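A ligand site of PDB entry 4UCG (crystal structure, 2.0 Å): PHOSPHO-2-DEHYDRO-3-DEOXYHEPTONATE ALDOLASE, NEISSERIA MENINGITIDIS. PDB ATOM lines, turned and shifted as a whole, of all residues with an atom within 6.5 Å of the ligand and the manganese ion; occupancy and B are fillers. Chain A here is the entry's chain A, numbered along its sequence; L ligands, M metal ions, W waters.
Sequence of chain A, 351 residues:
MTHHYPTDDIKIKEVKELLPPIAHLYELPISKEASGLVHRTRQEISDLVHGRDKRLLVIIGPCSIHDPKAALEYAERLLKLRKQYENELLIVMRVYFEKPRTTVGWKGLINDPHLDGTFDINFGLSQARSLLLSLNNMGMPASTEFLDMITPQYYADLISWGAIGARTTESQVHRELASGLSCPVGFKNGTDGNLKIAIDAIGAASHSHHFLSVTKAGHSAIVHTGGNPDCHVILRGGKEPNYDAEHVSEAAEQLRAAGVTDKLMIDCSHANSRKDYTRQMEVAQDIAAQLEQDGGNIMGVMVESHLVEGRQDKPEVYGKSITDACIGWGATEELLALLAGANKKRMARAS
NE2 of His 270 lies close to O1 of the ligand (3.2 Å).
An oxygen (O6) of the ligand is in salt-bridge range of the guanidinium group (NH1) of Arg 167, 2.8 Å away.
An oxygen (O1) of the ligand lies within salt-bridge range of the side-chain amino group (NZ) of Lys 99 (3.0 Å).
An oxygen (O4) of the ligand sits at hydrogen-bond distance from the backbone NH of Ala 166 (3.0 Å).
NH2 of Arg 94 lies within salt-bridge range of O1 of the ligand (2.8 Å).
NZ of Lys 188 lies within salt-bridge range of O5 of the ligand.
NE of Arg 236 lies within salt-bridge range of O5 of the ligand (2.8 Å).
N of Arg 236 lies close to ND2 of Asn 189 (3.0 Å).
N of Lys 188 is in hydrogen-bond range of O of Ile 164.
O of Cys 63 lies within hydrogen-bond range of NH2 of Arg 94 (3.0 Å).
NZ of Lys 99 is in hydrogen-bond range of O of Cys 63 (2.8 Å).
The backbone carbonyl oxygen (O) of Pro 62 lies within hydrogen-bond range of the guanidinium group (NE) of Arg 94, at 2.9 Å.
The backbone carbonyl oxygen (O) of Arg 236 sits at hydrogen-bond distance from the backbone NH (N) of Ala 271 (3.2 Å).
The side-chain carboxylate of Asp 267 lies within hydrogen-bond range of a ring nitrogen (ND1) of His 270 (2.6 Å).
The side-chain sulfur (SG) of Cys 63 sits close to the side-chain hydroxyl (OG1) of Thr 323, 3.0 Å away.
Tyr 96 touches the ligand (CE2 to O2, 3.6 Å).
OE1 of Glu 145 touches C3 of the ligand, at 3.6 Å.
Gly 165 touches the ligand.
Hydrophobic or aromatic side chains within 4 Å of the ligand: Tyr 96, Ala 166 and His 270.
11 residues have an atom within 4 Å of the ligand: Arg 94, Tyr 96, Lys 99, Glu 145, Gly 165, Ala 166, Arg 167, Lys 188, Arg 236, His 270 and Glu 304.
OD2 of Asp 324 is bound to the manganese ion.
OE2 of Glu 304 is bound to the manganese ion, 2.1 Å away.
The manganese ion is bound by water W1 (2.1 Å).
NE2 of His 270 is bound to the manganese ion, at 2.4 Å.
The side-chain sulfur (SG) of Cys 63 is bound to the manganese ion, at 2.6 Å.
The manganese ion has five donor atoms within binding distance.
Slightly farther from the manganese ion lies an oxygen (O1) of the ligand (2.8 Å).
Water W1 bridges O1 of the ligand and NZ of Lys 99.
Water W2 lies within hydrogen-bond range of OE1 of Glu 145 (2.6 Å) and O4 of the ligand (3.0 Å).
Water W3 lies within hydrogen-bond range of NH1 of Arg 167 (2.8 Å), O4 of the ligand (3.0 Å) and N of Ala 166 (3.2 Å).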
ATOM      1  N   PRO A  62      14.842 -25.338  14.476  1.00  0.00           N
ATOM      2  CA  PRO A  62      15.768 -24.719  15.414  1.00  0.00           C
ATOM      3  C   PRO A  62      17.102 -24.347  14.803  1.00  0.00           C
ATOM      4  O   PRO A  62      17.558 -24.987  13.872  1.00  0.00           O
ATOM      5  CB  PRO A  62      15.946 -25.800  16.472  1.00  0.00           C
ATOM      6  CG  PRO A  62      14.614 -26.508  16.471  1.00  0.00           C
ATOM      7  CD  PRO A  62      14.246 -26.578  15.023  1.00  0.00           C
ATOM      8  N   CYS A  63      17.741 -23.314  15.319  1.00  0.00           N
ATOM      9  CA  CYS A  63      19.144 -23.057  14.958  1.00  0.00           C
ATOM     10  C   CYS A  63      20.004 -24.294  15.242  1.00  0.00           C
ATOM     11  O   CYS A  63      20.777 -24.758  14.382  1.00  0.00           O
ATOM     12  CB  CYS A  63      19.677 -21.831  15.694  1.00  0.00           C
ATOM     13  SG  CYS A  63      21.435 -21.518  15.427  1.00  0.00           S
ATOM     14  N   SER A  64      19.807 -24.877  16.431  1.00  0.00           N
ATOM     15  CA  SER A  64      20.517 -26.074  16.847  1.00  0.00           C
ATOM     16  C   SER A  64      19.591 -26.963  17.609  1.00  0.00           C
ATOM     17  O   SER A  64      18.660 -26.475  18.269  1.00  0.00           O
ATOM     18  CB  SER A  64      21.675 -25.718  17.790  1.00  0.00           C
ATOM     19  OG  SER A  64      21.224 -24.962  18.909  1.00  0.00           O
ATOM     20  N   ARG A  94      14.834 -28.404  10.151  1.00  0.00           N
ATOM     21  CA  ARG A  94      16.237 -28.168  10.518  1.00  0.00           C
ATOM     22  C   ARG A  94      16.569 -29.020  11.727  1.00  0.00           C
ATOM     23  O   ARG A  94      15.942 -28.863  12.778  1.00  0.00           O
ATOM     24  CB  ARG A  94      16.497 -26.687  10.890  1.00  0.00           C
ATOM     25  CG  ARG A  94      16.630 -25.732   9.737  1.00  0.00           C
ATOM     26  CD  ARG A  94      16.795 -24.280  10.202  1.00  0.00           C
ATOM     27  NE  ARG A  94      17.933 -24.174  11.091  1.00  0.00           N
ATOM     28  CZ  ARG A  94      19.122 -23.705  10.752  1.00  0.00           C
ATOM     29  NH1 ARG A  94      19.342 -23.163   9.563  1.00  0.00           N
ATOM     30  NH2 ARG A  94      20.100 -23.737  11.632  1.00  0.00           N
ATOM     31  N   TYR A  96      19.942 -29.552  13.149  1.00  0.00           N
ATOM     32  CA  TYR A  96      21.354 -29.217  13.102  1.00  0.00           C
ATOM     33  C   TYR A  96      22.093 -29.678  14.363  1.00  0.00           C
ATOM     34  O   TYR A  96      21.732 -29.277  15.465  1.00  0.00           O
ATOM     35  CB  TYR A  96      21.511 -27.697  12.928  1.00  0.00           C
ATOM     36  CG  TYR A  96      21.332 -27.210  11.500  1.00  0.00           C
ATOM     37  CD1 TYR A  96      20.297 -27.695  10.679  1.00  0.00           C
ATOM     38  CD2 TYR A  96      22.193 -26.267  10.968  1.00  0.00           C
ATOM     39  CE1 TYR A  96      20.128 -27.205   9.383  1.00  0.00           C
ATOM     40  CE2 TYR A  96      22.053 -25.799   9.678  1.00  0.00           C
ATOM     41  CZ  TYR A  96      21.034 -26.248   8.895  1.00  0.00           C
ATOM     42  OH  TYR A  96      20.913 -25.767   7.613  1.00  0.00           O
ATOM     43  N   GLU A  98      25.708 -29.756  14.459  1.00  0.00           N
ATOM     44  CA  GLU A  98      27.074 -29.253  14.327  1.00  0.00           C
ATOM     45  C   GLU A  98      27.005 -27.751  14.031  1.00  0.00           C
ATOM     46  O   GLU A  98      26.422 -27.309  13.016  1.00  0.00           O
ATOM     47  CB  GLU A  98      27.803 -30.007  13.214  1.00  0.00           C
ATOM     48  CG  GLU A  98      27.824 -31.515  13.446  1.00  0.00           C
ATOM     49  CD  GLU A  98      28.493 -32.331  12.339  1.00  0.00           C
ATOM     50  OE1 GLU A  98      28.932 -31.761  11.311  1.00  0.00           O
ATOM     51  OE2 GLU A  98      28.555 -33.567  12.498  1.00  0.00           O
ATOM     52  N   LYS A  99      27.574 -26.973  14.951  1.00  0.00           N
ATOM     53  CA  LYS A  99      27.506 -25.519  14.927  1.00  0.00           C
ATOM     54  C   LYS A  99      28.897 -24.900  14.791  1.00  0.00           C
ATOM     55  O   LYS A  99      29.789 -25.138  15.610  1.00  0.00           O
ATOM     56  CB  LYS A  99      26.819 -24.995  16.172  1.00  0.00           C
ATOM     57  CG  LYS A  99      25.451 -25.603  16.407  1.00  0.00           C
ATOM     58  CD  LYS A  99      24.511 -25.421  15.219  1.00  0.00           C
ATOM     59  CE  LYS A  99      24.346 -23.950  14.877  1.00  0.00           C
ATOM     60  NZ  LYS A  99      23.373 -23.775  13.764  1.00  0.00           N
ATOM     61  N   PRO A 100      29.076 -24.082  13.757  1.00  0.00           N
ATOM     62  CA  PRO A 100      30.349 -23.409  13.575  1.00  0.00           C
ATOM     63  C   PRO A 100      30.371 -22.118  14.374  1.00  0.00           C
ATOM     64  O   PRO A 100      29.549 -21.256  14.139  1.00  0.00           O
ATOM     65  CB  PRO A 100      30.374 -23.135  12.078  1.00  0.00           C
ATOM     66  CG  PRO A 100      28.941 -22.986  11.690  1.00  0.00           C
ATOM     67  CD  PRO A 100      28.126 -23.790  12.670  1.00  0.00           C
ATOM     68  N   GLU A 145      23.588 -29.040   8.784  1.00  0.00           N
ATOM     69  CA  GLU A 145      24.864 -28.553   8.241  1.00  0.00           C
ATOM     70  C   GLU A 145      25.923 -29.619   8.471  1.00  0.00           C
ATOM     71  O   GLU A 145      26.167 -30.055   9.596  1.00  0.00           O
ATOM     72  CB  GLU A 145      25.360 -27.261   8.892  1.00  0.00           C
ATOM     73  CG  GLU A 145      26.802 -26.900   8.429  1.00  0.00           C
ATOM     74  CD  GLU A 145      27.371 -25.597   8.993  1.00  0.00           C
ATOM     75  OE1 GLU A 145      26.621 -24.736   9.582  1.00  0.00           O
ATOM     76  OE2 GLU A 145      28.617 -25.433   8.826  1.00  0.00           O
ATOM     77  N   ALA A 163      23.496 -28.635   4.381  1.00  0.00           N
ATOM     78  CA  ALA A 163      24.045 -27.311   4.206  1.00  0.00           C
ATOM     79  C   ALA A 163      25.553 -27.366   4.404  1.00  0.00           C
ATOM     80  O   ALA A 163      26.047 -28.146   5.239  1.00  0.00           O
ATOM     81  CB  ALA A 163      23.444 -26.368   5.216  1.00  0.00           C
ATOM     82  N   ILE A 164      26.265 -26.557   3.639  1.00  0.00           N
ATOM     83  CA  ILE A 164      27.647 -26.224   3.941  1.00  0.00           C
ATOM     84  C   ILE A 164      27.586 -24.763   4.300  1.00  0.00           C
ATOM     85  O   ILE A 164      27.125 -23.920   3.507  1.00  0.00           O
ATOM     86  CB  ILE A 164      28.587 -26.481   2.728  1.00  0.00           C
ATOM     87  CG1 ILE A 164      28.590 -27.965   2.358  1.00  0.00           C
ATOM     88  CG2 ILE A 164      30.001 -25.997   3.017  1.00  0.00           C
ATOM     89  CD1 ILE A 164      29.080 -28.928   3.414  1.00  0.00           C
ATOM     90  N   GLY A 165      28.047 -24.452   5.510  1.00  0.00           N
ATOM     91  CA  GLY A 165      27.884 -23.115   6.073  1.00  0.00           C
ATOM     92  C   GLY A 165      28.726 -22.022   5.425  1.00  0.00           C
ATOM     93  O   GLY A 165      29.681 -22.283   4.706  1.00  0.00           O
ATOM     94  N   ALA A 166      28.340 -20.787   5.703  1.00  0.00           N
ATOM     95  CA  ALA A 166      29.010 -19.632   5.175  1.00  0.00           C
ATOM     96  C   ALA A 166      30.526 -19.688   5.367  1.00  0.00           C
ATOM     97  O   ALA A 166      31.283 -19.288   4.474  1.00  0.00           O
ATOM     98  CB  ALA A 166      28.421 -18.380   5.801  1.00  0.00           C
ATOM     99  N   ARG A 167      30.952 -20.242   6.509  1.00  0.00           N
ATOM    100  CA  ARG A 167      32.339 -20.206   6.945  1.00  0.00           C
ATOM    101  C   ARG A 167      33.196 -21.318   6.375  1.00  0.00           C
ATOM    102  O   ARG A 167      34.394 -21.347   6.607  1.00  0.00           O
ATOM    103  CB  ARG A 167      32.395 -20.319   8.480  1.00  0.00           C
ATOM    104  CG  ARG A 167      31.770 -19.127   9.178  1.00  0.00           C
ATOM    105  CD  ARG A 167      31.627 -19.395  10.667  1.00  0.00           C
ATOM    106  NE  ARG A 167      30.876 -18.294  11.264  1.00  0.00           N
ATOM    107  CZ  ARG A 167      29.561 -18.113  11.139  1.00  0.00           C
ATOM    108  NH1 ARG A 167      28.777 -18.991  10.505  1.00  0.00           N
ATOM    109  NH2 ARG A 167      29.022 -17.041  11.704  1.00  0.00           N
ATOM    110  N   LYS A 188      26.235 -21.888   1.310  1.00  0.00           N
ATOM    111  CA  LYS A 188      25.932 -20.514   1.681  1.00  0.00           C
ATOM    112  C   LYS A 188      26.996 -19.578   1.121  1.00  0.00           C
ATOM    113  O   LYS A 188      28.180 -19.935   1.057  1.00  0.00           O
ATOM    114  CB  LYS A 188      25.840 -20.402   3.210  1.00  0.00           C
ATOM    115  CG  LYS A 188      24.584 -21.067   3.768  1.00  0.00           C
ATOM    116  CD  LYS A 188      24.295 -20.727   5.207  1.00  0.00           C
ATOM    117  CE  LYS A 188      22.791 -20.676   5.455  1.00  0.00           C
ATOM    118  NZ  LYS A 188      22.522 -20.229   6.833  1.00  0.00           N
ATOM    119  N   ASN A 189      26.580 -18.370   0.734  1.00  0.00           N
ATOM    120  CA  ASN A 189      27.536 -17.316   0.447  1.00  0.00           C
ATOM    121  C   ASN A 189      28.371 -17.026   1.677  1.00  0.00           C
ATOM    122  O   ASN A 189      27.982 -17.358   2.799  1.00  0.00           O
ATOM    123  CB  ASN A 189      26.877 -16.059  -0.107  1.00  0.00           C
ATOM    124  CG  ASN A 189      26.057 -15.305   0.933  1.00  0.00           C
ATOM    125  OD1 ASN A 189      26.595 -14.692   1.901  1.00  0.00           O
ATOM    126  ND2 ASN A 189      24.792 -15.310   0.730  1.00  0.00           N
ATOM    127  N   THR A 191      30.505 -15.084   4.746  1.00  0.00           N
ATOM    128  CA  THR A 191      29.954 -14.283   5.827  1.00  0.00           C
ATOM    129  C   THR A 191      29.952 -12.769   5.504  1.00  0.00           C
ATOM    130  O   THR A 191      29.171 -12.015   6.105  1.00  0.00           O
ATOM    131  CB  THR A 191      30.705 -14.514   7.148  1.00  0.00           C
ATOM    132  OG1 THR A 191      32.104 -14.308   6.952  1.00  0.00           O
ATOM    133  CG2 THR A 191      30.423 -15.914   7.690  1.00  0.00           C
ATOM    134  N   ARG A 236      22.308 -15.851   2.231  1.00  0.00           N
ATOM    135  CA  ARG A 236      22.156 -15.655   3.676  1.00  0.00           C
ATOM    136  C   ARG A 236      22.619 -14.298   4.212  1.00  0.00           C
ATOM    137  O   ARG A 236      22.758 -14.119   5.411  1.00  0.00           O
ATOM    138  CB  ARG A 236      22.823 -16.800   4.455  1.00  0.00           C
ATOM    139  CG  ARG A 236      24.248 -17.113   4.024  1.00  0.00           C
ATOM    140  CD  ARG A 236      25.229 -16.113   4.618  1.00  0.00           C
ATOM    141  NE  ARG A 236      25.408 -16.292   6.053  1.00  0.00           N
ATOM    142  CZ  ARG A 236      25.984 -15.400   6.844  1.00  0.00           C
ATOM    143  NH1 ARG A 236      26.443 -14.261   6.349  1.00  0.00           N
ATOM    144  NH2 ARG A 236      26.110 -15.644   8.141  1.00  0.00           N
ATOM    145  N   ASP A 267      17.953 -17.668   2.763  1.00  0.00           N
ATOM    146  CA  ASP A 267      17.871 -17.767   4.227  1.00  0.00           C
ATOM    147  C   ASP A 267      17.232 -16.494   4.751  1.00  0.00           C
ATOM    148  O   ASP A 267      17.731 -15.408   4.482  1.00  0.00           O
ATOM    149  CB  ASP A 267      19.286 -17.953   4.811  1.00  0.00           C
ATOM    150  CG  ASP A 267      19.304 -18.231   6.316  1.00  0.00           C
ATOM    151  OD1 ASP A 267      18.240 -18.271   6.947  1.00  0.00           O
ATOM    152  OD2 ASP A 267      20.415 -18.392   6.873  1.00  0.00           O
ATOM    153  N   SER A 269      17.087 -15.852   7.882  1.00  0.00           N
ATOM    154  CA  SER A 269      17.785 -15.623   9.148  1.00  0.00           C
ATOM    155  C   SER A 269      19.223 -15.117   8.980  1.00  0.00           C
ATOM    156  O   SER A 269      19.595 -14.619   7.930  1.00  0.00           O
ATOM    157  CB  SER A 269      17.752 -16.871  10.025  1.00  0.00           C
ATOM    158  OG  SER A 269      17.816 -16.531  11.388  1.00  0.00           O
ATOM    159  N   HIS A 270      20.007 -15.242  10.054  1.00  0.00           N
ATOM    160  CA  HIS A 270      21.393 -14.822  10.036  1.00  0.00           C
ATOM    161  C   HIS A 270      21.572 -13.404   9.471  1.00  0.00           C
ATOM    162  O   HIS A 270      20.903 -12.475   9.932  1.00  0.00           O
ATOM    163  CB  HIS A 270      22.247 -15.895   9.341  1.00  0.00           C
ATOM    164  CG  HIS A 270      22.002 -17.241   9.915  1.00  0.00           C
ATOM    165  ND1 HIS A 270      21.156 -18.153   9.332  1.00  0.00           N
ATOM    166  CD2 HIS A 270      22.359 -17.762  11.113  1.00  0.00           C
ATOM    167  CE1 HIS A 270      21.049 -19.210  10.118  1.00  0.00           C
ATOM    168  NE2 HIS A 270      21.788 -19.007  11.187  1.00  0.00           N
ATOM    169  N   ALA A 271      22.456 -13.203   8.504  1.00  0.00           N
ATOM    170  CA  ALA A 271      22.780 -11.851   8.055  1.00  0.00           C
ATOM    171  C   ALA A 271      21.635 -11.230   7.250  1.00  0.00           C
ATOM    172  O   ALA A 271      21.600 -10.030   7.078  1.00  0.00           O
ATOM    173  CB  ALA A 271      24.088 -11.821   7.284  1.00  0.00           C
ATOM    174  N   MET A 302      14.932 -20.687   3.985  1.00  0.00           N
ATOM    175  CA  MET A 302      15.406 -21.194   5.258  1.00  0.00           C
ATOM    176  C   MET A 302      14.935 -20.277   6.379  1.00  0.00           C
ATOM    177  O   MET A 302      14.910 -19.040   6.220  1.00  0.00           O
ATOM    178  CB  MET A 302      16.934 -21.303   5.232  1.00  0.00           C
ATOM    179  CG  MET A 302      17.567 -21.924   6.472  1.00  0.00           C
ATOM    180  SD  MET A 302      19.406 -22.039   6.329  1.00  0.00           S
ATOM    181  CE  MET A 302      19.541 -22.748   4.726  1.00  0.00           C
ATOM    182  N   GLU A 304      14.709 -19.938  10.865  1.00  0.00           N
ATOM    183  CA  GLU A 304      15.097 -20.421  12.173  1.00  0.00           C
ATOM    184  C   GLU A 304      13.907 -20.225  13.131  1.00  0.00           C
ATOM    185  O   GLU A 304      13.550 -19.097  13.435  1.00  0.00           O
ATOM    186  CB  GLU A 304      16.344 -19.673  12.630  1.00  0.00           C
ATOM    187  CG  GLU A 304      17.590 -20.155  11.911  1.00  0.00           C
ATOM    188  CD  GLU A 304      18.872 -19.698  12.579  1.00  0.00           C
ATOM    189  OE1 GLU A 304      18.999 -18.504  12.848  1.00  0.00           O
ATOM    190  OE2 GLU A 304      19.777 -20.544  12.792  1.00  0.00           O
ATOM    191  N   THR A 323      21.281 -21.290  20.877  1.00  0.00           N
ATOM    192  CA  THR A 323      22.158 -20.662  19.871  1.00  0.00           C
ATOM    193  C   THR A 323      21.456 -19.405  19.294  1.00  0.00           C
ATOM    194  O   THR A 323      21.025 -18.540  20.081  1.00  0.00           O
ATOM    195  CB  THR A 323      22.683 -21.681  18.828  1.00  0.00           C
ATOM    196  OG1 THR A 323      21.611 -22.455  18.271  1.00  0.00           O
ATOM    197  CG2 THR A 323      23.650 -22.616  19.518  1.00  0.00           C
ATOM    198  N   ASP A 324      21.305 -19.282  17.983  1.00  0.00           N
ATOM    199  CA  ASP A 324      20.671 -18.075  17.450  1.00  0.00           C
ATOM    200  C   ASP A 324      19.209 -18.003  17.873  1.00  0.00           C
ATOM    201  O   ASP A 324      18.517 -19.027  17.961  1.00  0.00           O
ATOM    202  CB  ASP A 324      20.740 -18.012  15.918  1.00  0.00           C
ATOM    203  CG  ASP A 324      22.162 -17.974  15.386  1.00  0.00           C
ATOM    204  OD1 ASP A 324      23.041 -17.414  16.076  1.00  0.00           O
ATOM    205  OD2 ASP A 324      22.398 -18.540  14.289  1.00  0.00           O
HETATM  206  C1  LIG L   1      22.825 -21.943  10.298  1.00  0.00           C
HETATM  207  O1  LIG L   1      22.400 -22.153  11.451  1.00  0.00           O
HETATM  208  O2  LIG L   1      22.123 -22.221   9.281  1.00  0.00           O
HETATM  209  C2  LIG L   1      24.174 -21.356  10.106  1.00  0.00           C
HETATM  210  C3  LIG L   1      25.229 -21.674  10.829  1.00  0.00           C
HETATM  211  O3  LIG L   1      24.227 -20.372   9.029  1.00  0.00           O
HETATM  212  P1  LIG L   1      25.472 -19.486   8.515  1.00  0.00           P
HETATM  213  O4  LIG L   1      26.391 -20.562   7.977  1.00  0.00           O
HETATM  214  O5  LIG L   1      24.729 -18.484   7.705  1.00  0.00           O
HETATM  215  O6  LIG L   1      26.047 -18.862   9.804  1.00  0.00           O
HETATM  216 MN    MN M   1      21.741 -20.146  13.277  1.00  0.00          MN
HETATM  217  O   HOH W   1      23.599 -21.093  13.374  1.00  0.00           O
HETATM  218  O   HOH W   2      25.235 -23.304   7.862  1.00  0.00           O
HETATM  219  O   HOH W   3      29.242 -21.097   8.772  1.00  0.00           O
